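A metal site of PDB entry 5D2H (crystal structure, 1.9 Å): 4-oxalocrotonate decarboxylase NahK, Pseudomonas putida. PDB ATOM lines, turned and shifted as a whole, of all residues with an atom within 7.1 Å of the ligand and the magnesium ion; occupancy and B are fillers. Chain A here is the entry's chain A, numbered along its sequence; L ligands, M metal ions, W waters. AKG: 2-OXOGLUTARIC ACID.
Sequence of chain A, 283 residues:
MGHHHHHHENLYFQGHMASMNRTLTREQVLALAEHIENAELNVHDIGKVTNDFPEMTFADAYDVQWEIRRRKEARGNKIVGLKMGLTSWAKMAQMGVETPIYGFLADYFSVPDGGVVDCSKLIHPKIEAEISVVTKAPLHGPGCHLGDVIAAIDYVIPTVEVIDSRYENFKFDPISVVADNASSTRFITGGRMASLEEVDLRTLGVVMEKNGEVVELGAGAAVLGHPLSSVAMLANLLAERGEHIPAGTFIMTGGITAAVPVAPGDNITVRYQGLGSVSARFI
Lys 83 touches the magnesium ion. Met 84 touches the magnesium ion. Within 4 Å of the magnesium ion: Lys 83, Met 84, Glu 128, Glu 130 and Glu 161.
Water W3 bridges OE2 of Glu 130 (2.6 Å) and O of Met 84 (2.6 Å). Water W5 lies within hydrogen-bond range of an oxygen (O1) of the ligand (2.5 Å), the backbone NH of Gly 255 (2.8 Å), the side-chain carboxylate of Glu 128 (3.0 Å) and the backbone carbonyl oxygen of Met 84 (3.4 Å). Water W1 lies within hydrogen-bond range of the side-chain carboxylate of Glu 128 (2.6 Å) and an oxygen (O4) of the ligand (3.3 Å). Water W2 lies within hydrogen-bond range of the side-chain hydroxyl (OG1) of Thr 87 (2.5 Å), the backbone NH (N) of Gly 255 (3.1 Å), an oxygen (O1) of the ligand (3.4 Å) and the backbone carbonyl oxygen (O) of Met 84 (3.5 Å).
OE2 of Glu 128 binds the magnesium ion. OE1 of Glu 130 is bound to the magnesium ion. The side-chain carboxylate (OE1) of Glu 161 binds the magnesium ion (2.0 Å). The magnesium ion is bound by water W3 (2.0 Å). The magnesium ion is bound by water W5 (2.1 Å). An oxygen (O2) of the ligand is bound to the magnesium ion (2.4 Å). The magnesium ion has six donor atoms within binding distance.
OE2 of Glu 130 sits at hydrogen-bond distance from N of Gly 254 (2.9 Å). OE2 of Glu 161 is in salt-bridge range of NZ of Lys 83 (2.6 Å). The backbone carbonyl oxygen of Ala 182 lies within hydrogen-bond range of the side-chain amino group of Lys 83 (2.9 Å). The side-chain hydroxyl (OG) of Ser 184 sits close to the side-chain amino group (NZ) of Lys 83, at 3.3 Å. The backbone NH (N) of Ala 182 lies within hydrogen-bond range of the backbone carbonyl oxygen (O) of Val 177, 2.7 Å away. The backbone carbonyl oxygen (O) of Ile 101 is in hydrogen-bond range of the backbone NH (N) of Gly 85. N of Lys 91 sits at hydrogen-bond distance from OG of Ser 88 (3.0 Å). O of Ser 183 lies within hydrogen-bond range of N of Asp 164 (2.8 Å).
NZ of Lys 83 sits close to O2 of the ligand (2.8 Å). N of Leu 86 is in hydrogen-bond range of O3 of the ligand.
O of Ala 182 sits close to O5 of the ligand (2.8 Å). Residues that only touch the ligand: Gly 85 (3.4 Å), Lys 91 (3.5 Å), Phe 172 (3.6 Å), Ile 163 (3.6 Å), Ser 183 (3.6 Å) and Met 84 (3.6 Å). Hydrophobic or aromatic side chains that line the ligand: Leu 86, Ile 163 and Phe 172. Within 4 Å of the ligand: Lys 83, Met 84, Gly 85, Leu 86, Lys 91, Glu 128, Glu 161, Ile 163, Phe 172, Ala 182 and Ser 183. Along chain A the residues within 4 Å of the ligand span positions 83 to 183.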
ATOM      1  N   LYS A  83       2.209 -23.733  33.775  1.00  0.00           N
ATOM      2  CA  LYS A  83       2.512 -22.860  32.661  1.00  0.00           C
ATOM      3  C   LYS A  83       2.744 -23.705  31.436  1.00  0.00           C
ATOM      4  O   LYS A  83       3.038 -24.901  31.566  1.00  0.00           O
ATOM      5  CB  LYS A  83       3.692 -21.927  32.963  1.00  0.00           C
ATOM      6  CG  LYS A  83       4.977 -22.595  33.440  1.00  0.00           C
ATOM      7  CD  LYS A  83       5.687 -23.323  32.319  1.00  0.00           C
ATOM      8  CE  LYS A  83       6.165 -22.360  31.240  1.00  0.00           C
ATOM      9  NZ  LYS A  83       7.363 -21.566  31.654  1.00  0.00           N
ATOM     10  N   MET A  84       2.559 -23.123  30.263  1.00  0.00           N
ATOM     11  CA  MET A  84       2.696 -23.864  29.017  1.00  0.00           C
ATOM     12  C   MET A  84       3.874 -23.327  28.239  1.00  0.00           C
ATOM     13  O   MET A  84       4.058 -22.117  28.157  1.00  0.00           O
ATOM     14  CB  MET A  84       1.448 -23.737  28.151  1.00  0.00           C
ATOM     15  CG  MET A  84       0.194 -24.212  28.809  1.00  0.00           C
ATOM     16  SD  MET A  84       0.405 -25.924  29.244  1.00  0.00           S
ATOM     17  CE  MET A  84       0.403 -26.724  27.644  1.00  0.00           C
ATOM     18  N   GLY A  85       4.657 -24.235  27.669  1.00  0.00           N
ATOM     19  CA  GLY A  85       5.743 -23.852  26.788  1.00  0.00           C
ATOM     20  C   GLY A  85       5.550 -24.433  25.403  1.00  0.00           C
ATOM     21  O   GLY A  85       4.794 -25.404  25.230  1.00  0.00           O
ATOM     22  N   LEU A  86       6.235 -23.862  24.415  1.00  0.00           N
ATOM     23  CA  LEU A  86       6.174 -24.375  23.048  1.00  0.00           C
ATOM     24  C   LEU A  86       4.729 -24.355  22.539  1.00  0.00           C
ATOM     25  O   LEU A  86       4.234 -25.346  22.012  1.00  0.00           O
ATOM     26  CB  LEU A  86       6.721 -25.802  22.994  1.00  0.00           C
ATOM     27  CG  LEU A  86       8.228 -25.908  23.239  1.00  0.00           C
ATOM     28  CD1 LEU A  86       8.672 -27.347  23.069  1.00  0.00           C
ATOM     29  CD2 LEU A  86       8.960 -24.990  22.280  1.00  0.00           C
ATOM     30  N   THR A  87       4.065 -23.225  22.735  1.00  0.00           N
ATOM     31  CA  THR A  87       2.669 -23.085  22.340  1.00  0.00           C
ATOM     32  C   THR A  87       2.611 -22.425  20.980  1.00  0.00           C
ATOM     33  O   THR A  87       1.758 -21.594  20.710  1.00  0.00           O
ATOM     34  CB  THR A  87       1.893 -22.187  23.324  1.00  0.00           C
ATOM     35  OG1 THR A  87       2.601 -20.963  23.504  1.00  0.00           O
ATOM     36  CG2 THR A  87       1.712 -22.895  24.664  1.00  0.00           C
ATOM     37  N   SER A  88       3.566 -22.794  20.128  1.00  0.00           N
ATOM     38  CA  SER A  88       3.624 -22.273  18.783  1.00  0.00           C
ATOM     39  C   SER A  88       3.810 -23.433  17.828  1.00  0.00           C
ATOM     40  O   SER A  88       4.744 -24.229  17.985  1.00  0.00           O
ATOM     41  CB  SER A  88       4.803 -21.309  18.636  1.00  0.00           C
ATOM     42  OG  SER A  88       5.170 -21.163  17.280  1.00  0.00           O
ATOM     43  N   LYS A  91       7.145 -23.282  16.326  1.00  0.00           N
ATOM     44  CA  LYS A  91       8.239 -23.612  17.226  1.00  0.00           C
ATOM     45  C   LYS A  91       8.264 -25.111  17.510  1.00  0.00           C
ATOM     46  O   LYS A  91       9.331 -25.715  17.598  1.00  0.00           O
ATOM     47  CB  LYS A  91       8.168 -22.803  18.530  1.00  0.00           C
ATOM     48  CG  LYS A  91       9.519 -22.637  19.219  1.00  0.00           C
ATOM     49  CD  LYS A  91       9.381 -22.062  20.633  1.00  0.00           C
ATOM     50  CE  LYS A  91      10.760 -21.770  21.266  1.00  0.00           C
ATOM     51  NZ  LYS A  91      11.301 -20.410  20.908  1.00  0.00           N
ATOM     52  N   MET A  95      11.380 -27.465  16.846  1.00  0.00           N
ATOM     53  CA  MET A  95      12.008 -28.262  17.902  1.00  0.00           C
ATOM     54  C   MET A  95      11.757 -29.761  17.740  1.00  0.00           C
ATOM     55  O   MET A  95      12.230 -30.562  18.546  1.00  0.00           O
ATOM     56  CB  MET A  95      11.550 -27.810  19.281  1.00  0.00           C
ATOM     57  CG  MET A  95      11.821 -26.358  19.563  1.00  0.00           C
ATOM     58  SD  MET A  95      13.528 -25.926  19.159  1.00  0.00           S
ATOM     59  CE  MET A  95      13.473 -24.154  19.330  1.00  0.00           C
ATOM     60  N   ILE A 101       4.724 -28.092  25.905  1.00  0.00           N
ATOM     61  CA  ILE A 101       5.209 -28.676  27.125  1.00  0.00           C
ATOM     62  C   ILE A 101       4.613 -27.840  28.239  1.00  0.00           C
ATOM     63  O   ILE A 101       4.078 -26.759  27.983  1.00  0.00           O
ATOM     64  CB  ILE A 101       6.737 -28.602  27.229  1.00  0.00           C
ATOM     65  CG1 ILE A 101       7.194 -27.150  27.118  1.00  0.00           C
ATOM     66  CG2 ILE A 101       7.386 -29.452  26.136  1.00  0.00           C
ATOM     67  CD1 ILE A 101       8.661 -26.961  27.455  1.00  0.00           C
ATOM     68  N   GLU A 128       7.981 -12.801  29.121  1.00  0.00           N
ATOM     69  CA  GLU A 128       7.051 -12.985  28.031  1.00  0.00           C
ATOM     70  C   GLU A 128       5.652 -12.567  28.475  1.00  0.00           C
ATOM     71  O   GLU A 128       5.299 -12.706  29.657  1.00  0.00           O
ATOM     72  CB  GLU A 128       7.075 -14.434  27.524  1.00  0.00           C
ATOM     73  CG  GLU A 128       7.110 -15.468  28.608  1.00  0.00           C
ATOM     74  CD  GLU A 128       7.313 -16.871  28.071  1.00  0.00           C
ATOM     75  OE1 GLU A 128       7.558 -17.053  26.855  1.00  0.00           O
ATOM     76  OE2 GLU A 128       7.226 -17.820  28.877  1.00  0.00           O
ATOM     77  N   ALA A 129       4.888 -12.029  27.537  1.00  0.00           N
ATOM     78  CA  ALA A 129       3.508 -11.620  27.767  1.00  0.00           C
ATOM     79  C   ALA A 129       2.578 -12.787  27.512  1.00  0.00           C
ATOM     80  O   ALA A 129       2.638 -13.410  26.447  1.00  0.00           O
ATOM     81  CB  ALA A 129       3.137 -10.453  26.873  1.00  0.00           C
ATOM     82  N   GLU A 130       1.729 -13.081  28.487  1.00  0.00           N
ATOM     83  CA  GLU A 130       0.837 -14.216  28.375  1.00  0.00           C
ATOM     84  C   GLU A 130      -0.527 -13.836  28.888  1.00  0.00           C
ATOM     85  O   GLU A 130      -0.716 -12.806  29.553  1.00  0.00           O
ATOM     86  CB  GLU A 130       1.387 -15.415  29.160  1.00  0.00           C
ATOM     87  CG  GLU A 130       2.849 -15.716  28.904  1.00  0.00           C
ATOM     88  CD  GLU A 130       3.266 -17.133  29.297  1.00  0.00           C
ATOM     89  OE1 GLU A 130       4.482 -17.362  29.471  1.00  0.00           O
ATOM     90  OE2 GLU A 130       2.408 -18.035  29.418  1.00  0.00           O
ATOM     91  N   GLU A 161       5.328 -13.734  32.285  1.00  0.00           N
ATOM     92  CA  GLU A 161       6.172 -14.745  32.894  1.00  0.00           C
ATOM     93  C   GLU A 161       7.603 -14.282  32.829  1.00  0.00           C
ATOM     94  O   GLU A 161       8.020 -13.644  31.864  1.00  0.00           O
ATOM     95  CB  GLU A 161       6.021 -16.111  32.222  1.00  0.00           C
ATOM     96  CG  GLU A 161       6.684 -17.215  33.049  1.00  0.00           C
ATOM     97  CD  GLU A 161       6.578 -18.621  32.464  1.00  0.00           C
ATOM     98  OE1 GLU A 161       6.227 -18.781  31.283  1.00  0.00           O
ATOM     99  OE2 GLU A 161       6.868 -19.574  33.219  1.00  0.00           O
ATOM    100  N   VAL A 162       8.355 -14.559  33.885  1.00  0.00           N
ATOM    101  CA  VAL A 162       9.795 -14.461  33.799  1.00  0.00           C
ATOM    102  C   VAL A 162      10.299 -15.881  33.698  1.00  0.00           C
ATOM    103  O   VAL A 162      10.084 -16.701  34.595  1.00  0.00           O
ATOM    104  CB  VAL A 162      10.417 -13.718  35.005  1.00  0.00           C
ATOM    105  CG1 VAL A 162      11.917 -13.525  34.790  1.00  0.00           C
ATOM    106  CG2 VAL A 162       9.735 -12.356  35.186  1.00  0.00           C
ATOM    107  N   ILE A 163      10.914 -16.193  32.563  1.00  0.00           N
ATOM    108  CA  ILE A 163      11.466 -17.512  32.381  1.00  0.00           C
ATOM    109  C   ILE A 163      12.971 -17.395  32.473  1.00  0.00           C
ATOM    110  O   ILE A 163      13.540 -16.361  32.198  1.00  0.00           O
ATOM    111  CB  ILE A 163      11.045 -18.141  31.042  1.00  0.00           C
ATOM    112  CG1 ILE A 163      11.481 -17.240  29.873  1.00  0.00           C
ATOM    113  CG2 ILE A 163       9.525 -18.437  31.048  1.00  0.00           C
ATOM    114  CD1 ILE A 163      11.200 -17.839  28.511  1.00  0.00           C
ATOM    115  N   ASP A 164      13.603 -18.475  32.907  1.00  0.00           N
ATOM    116  CA  ASP A 164      15.024 -18.422  33.166  1.00  0.00           C
ATOM    117  C   ASP A 164      15.500 -19.850  33.119  1.00  0.00           C
ATOM    118  O   ASP A 164      15.401 -20.591  34.095  1.00  0.00           O
ATOM    119  CB  ASP A 164      15.276 -17.797  34.542  1.00  0.00           C
ATOM    120  CG  ASP A 164      16.744 -17.488  34.800  1.00  0.00           C
ATOM    121  OD1 ASP A 164      17.482 -17.244  33.825  1.00  0.00           O
ATOM    122  OD2 ASP A 164      17.159 -17.493  35.978  1.00  0.00           O
ATOM    123  N   SER A 165      15.982 -20.264  31.952  1.00  0.00           N
ATOM    124  CA  SER A 165      16.499 -21.591  31.792  1.00  0.00           C
ATOM    125  C   SER A 165      17.706 -21.724  32.714  1.00  0.00           C
ATOM    126  O   SER A 165      18.563 -20.839  32.728  1.00  0.00           O
ATOM    127  CB  SER A 165      16.934 -21.832  30.355  1.00  0.00           C
ATOM    128  OG  SER A 165      17.472 -23.125  30.230  1.00  0.00           O
ATOM    129  N   PHE A 172      17.925 -24.300  22.282  1.00  0.00           N
ATOM    130  CA  PHE A 172      16.776 -24.829  23.005  1.00  0.00           C
ATOM    131  C   PHE A 172      16.664 -26.353  22.873  1.00  0.00           C
ATOM    132  O   PHE A 172      16.701 -26.905  21.765  1.00  0.00           O
ATOM    133  CB  PHE A 172      15.499 -24.177  22.465  1.00  0.00           C
ATOM    134  CG  PHE A 172      14.268 -24.522  23.234  1.00  0.00           C
ATOM    135  CD1 PHE A 172      13.864 -23.737  24.295  1.00  0.00           C
ATOM    136  CD2 PHE A 172      13.501 -25.620  22.884  1.00  0.00           C
ATOM    137  CE1 PHE A 172      12.720 -24.040  25.020  1.00  0.00           C
ATOM    138  CE2 PHE A 172      12.359 -25.943  23.600  1.00  0.00           C
ATOM    139  CZ  PHE A 172      11.959 -25.145  24.666  1.00  0.00           C
ATOM    140  N   VAL A 177      14.535 -28.764  28.790  1.00  0.00           N
ATOM    141  CA  VAL A 177      13.699 -27.664  29.275  1.00  0.00           C
ATOM    142  C   VAL A 177      12.588 -28.223  30.157  1.00  0.00           C
ATOM    143  O   VAL A 177      12.316 -27.681  31.228  1.00  0.00           O
ATOM    144  CB  VAL A 177      13.175 -26.797  28.119  1.00  0.00           C
ATOM    145  CG1 VAL A 177      12.066 -25.869  28.599  1.00  0.00           C
ATOM    146  CG2 VAL A 177      14.323 -25.985  27.512  1.00  0.00           C
ATOM    147  N   ASN A 181      11.660 -27.749  34.430  1.00  0.00           N
ATOM    148  CA  ASN A 181      10.361 -27.122  34.727  1.00  0.00           C
ATOM    149  C   ASN A 181       9.986 -26.049  33.704  1.00  0.00           C
ATOM    150  O   ASN A 181       9.463 -24.986  34.065  1.00  0.00           O
ATOM    151  CB  ASN A 181      10.342 -26.528  36.138  1.00  0.00           C
ATOM    152  CG  ASN A 181       8.939 -26.210  36.616  1.00  0.00           C
ATOM    153  OD1 ASN A 181       7.960 -26.860  36.212  1.00  0.00           O
ATOM    154  ND2 ASN A 181       8.817 -25.210  37.481  1.00  0.00           N
ATOM    155  N   ALA A 182      10.262 -26.325  32.432  1.00  0.00           N
ATOM    156  CA  ALA A 182       9.915 -25.389  31.378  1.00  0.00           C
ATOM    157  C   ALA A 182      10.474 -23.994  31.693  1.00  0.00           C
ATOM    158  O   ALA A 182       9.862 -22.978  31.360  1.00  0.00           O
ATOM    159  CB  ALA A 182       8.395 -25.339  31.197  1.00  0.00           C
ATOM    160  N   SER A 183      11.623 -23.959  32.366  1.00  0.00           N
ATOM    161  CA  SER A 183      12.329 -22.691  32.611  1.00  0.00           C
ATOM    162  C   SER A 183      11.557 -21.713  33.497  1.00  0.00           C
ATOM    163  O   SER A 183      11.832 -20.510  33.524  1.00  0.00           O
ATOM    164  CB  SER A 183      12.666 -22.010  31.276  1.00  0.00           C
ATOM    165  OG  SER A 183      13.296 -22.926  30.388  1.00  0.00           O
ATOM    166  N   SER A 184      10.577 -22.215  34.238  1.00  0.00           N
ATOM    167  CA  SER A 184       9.746 -21.314  35.041  1.00  0.00           C
ATOM    168  C   SER A 184      10.604 -20.699  36.145  1.00  0.00           C
ATOM    169  O   SER A 184      11.579 -21.311  36.589  1.00  0.00           O
ATOM    170  CB  SER A 184       8.567 -22.055  35.650  1.00  0.00           C
ATOM    171  OG  SER A 184       7.905 -22.833  34.663  1.00  0.00           O
ATOM    172  N   MET A 252      -0.965 -20.435  32.909  1.00  0.00           N
ATOM    173  CA  MET A 252      -0.389 -19.478  31.972  1.00  0.00           C
ATOM    174  C   MET A 252      -0.332 -20.125  30.589  1.00  0.00           C
ATOM    175  O   MET A 252       0.360 -21.107  30.401  1.00  0.00           O
ATOM    176  CB  MET A 252       0.998 -19.057  32.442  1.00  0.00           C
ATOM    177  CG  MET A 252       0.986 -18.541  33.883  1.00  0.00           C
ATOM    178  SD  MET A 252       2.580 -17.865  34.392  1.00  0.00           S
ATOM    179  CE  MET A 252       2.827 -16.731  33.028  1.00  0.00           C
ATOM    180  N   THR A 253      -1.075 -19.576  29.631  1.00  0.00           N
ATOM    181  CA  THR A 253      -1.367 -20.309  28.386  1.00  0.00           C
ATOM    182  C   THR A 253      -0.272 -20.261  27.322  1.00  0.00           C
ATOM    183  O   THR A 253      -0.321 -21.030  26.367  1.00  0.00           O
ATOM    184  CB  THR A 253      -2.722 -19.875  27.756  1.00  0.00           C
ATOM    185  OG1 THR A 253      -2.683 -18.488  27.416  1.00  0.00           O
ATOM    186  CG2 THR A 253      -3.877 -20.148  28.715  1.00  0.00           C
ATOM    187  N   GLY A 254       0.705 -19.380  27.477  1.00  0.00           N
ATOM    188  CA  GLY A 254       1.840 -19.370  26.589  1.00  0.00           C
ATOM    189  C   GLY A 254       2.302 -17.989  26.138  1.00  0.00           C
ATOM    190  O   GLY A 254       1.557 -17.020  26.204  1.00  0.00           O
ATOM    191  N   GLY A 255       3.554 -17.923  25.682  1.00  0.00           N
ATOM    192  CA  GLY A 255       4.135 -16.665  25.242  1.00  0.00           C
ATOM    193  C   GLY A 255       3.420 -16.111  24.031  1.00  0.00           C
ATOM    194  O   GLY A 255       3.383 -16.754  22.977  1.00  0.00           O
ATOM    195  N   ALA A 259      10.186 -13.821  23.699  1.00  0.00           N
ATOM    196  CA  ALA A 259      10.710 -13.538  25.027  1.00  0.00           C
ATOM    197  C   ALA A 259      11.793 -12.470  24.936  1.00  0.00           C
ATOM    198  O   ALA A 259      12.550 -12.417  23.973  1.00  0.00           O
ATOM    199  CB  ALA A 259      11.248 -14.799  25.687  1.00  0.00           C
HETATM  200  C1  AKG L   1       7.885 -20.988  28.001  1.00  0.00           C
HETATM  201  O1  AKG L   1       7.441 -20.675  26.875  1.00  0.00           O
HETATM  202  O2  AKG L   1       7.256 -20.670  29.052  1.00  0.00           O
HETATM  203  C2  AKG L   1       9.163 -21.699  28.119  1.00  0.00           C
HETATM  204  O5  AKG L   1       9.896 -21.398  29.050  1.00  0.00           O
HETATM  205  C3  AKG L   1       9.668 -22.790  27.197  1.00  0.00           C
HETATM  206  C4  AKG L   1       8.883 -22.984  25.911  1.00  0.00           C
HETATM  207  C5  AKG L   1       9.178 -21.952  24.837  1.00  0.00           C
HETATM  208  O3  AKG L   1       8.228 -21.684  24.071  1.00  0.00           O
HETATM  209  O4  AKG L   1      10.318 -21.412  24.747  1.00  0.00           O
HETATM  210 MG    MG M   1       5.737 -18.892  29.357  1.00  0.00          MG
HETATM  211  O   HOH W   1       9.208 -18.388  25.327  1.00  0.00           O
HETATM  212  O   HOH W   2       4.621 -20.717  25.033  1.00  0.00           O
HETATM  213  O   HOH W   3       4.105 -20.013  29.742  1.00  0.00           O
HETATM  214  O   HOH W   4      12.347 -20.480  25.954  1.00  0.00           O
HETATM  215  O   HOH W   5       5.490 -19.171  27.288  1.00  0.00           O
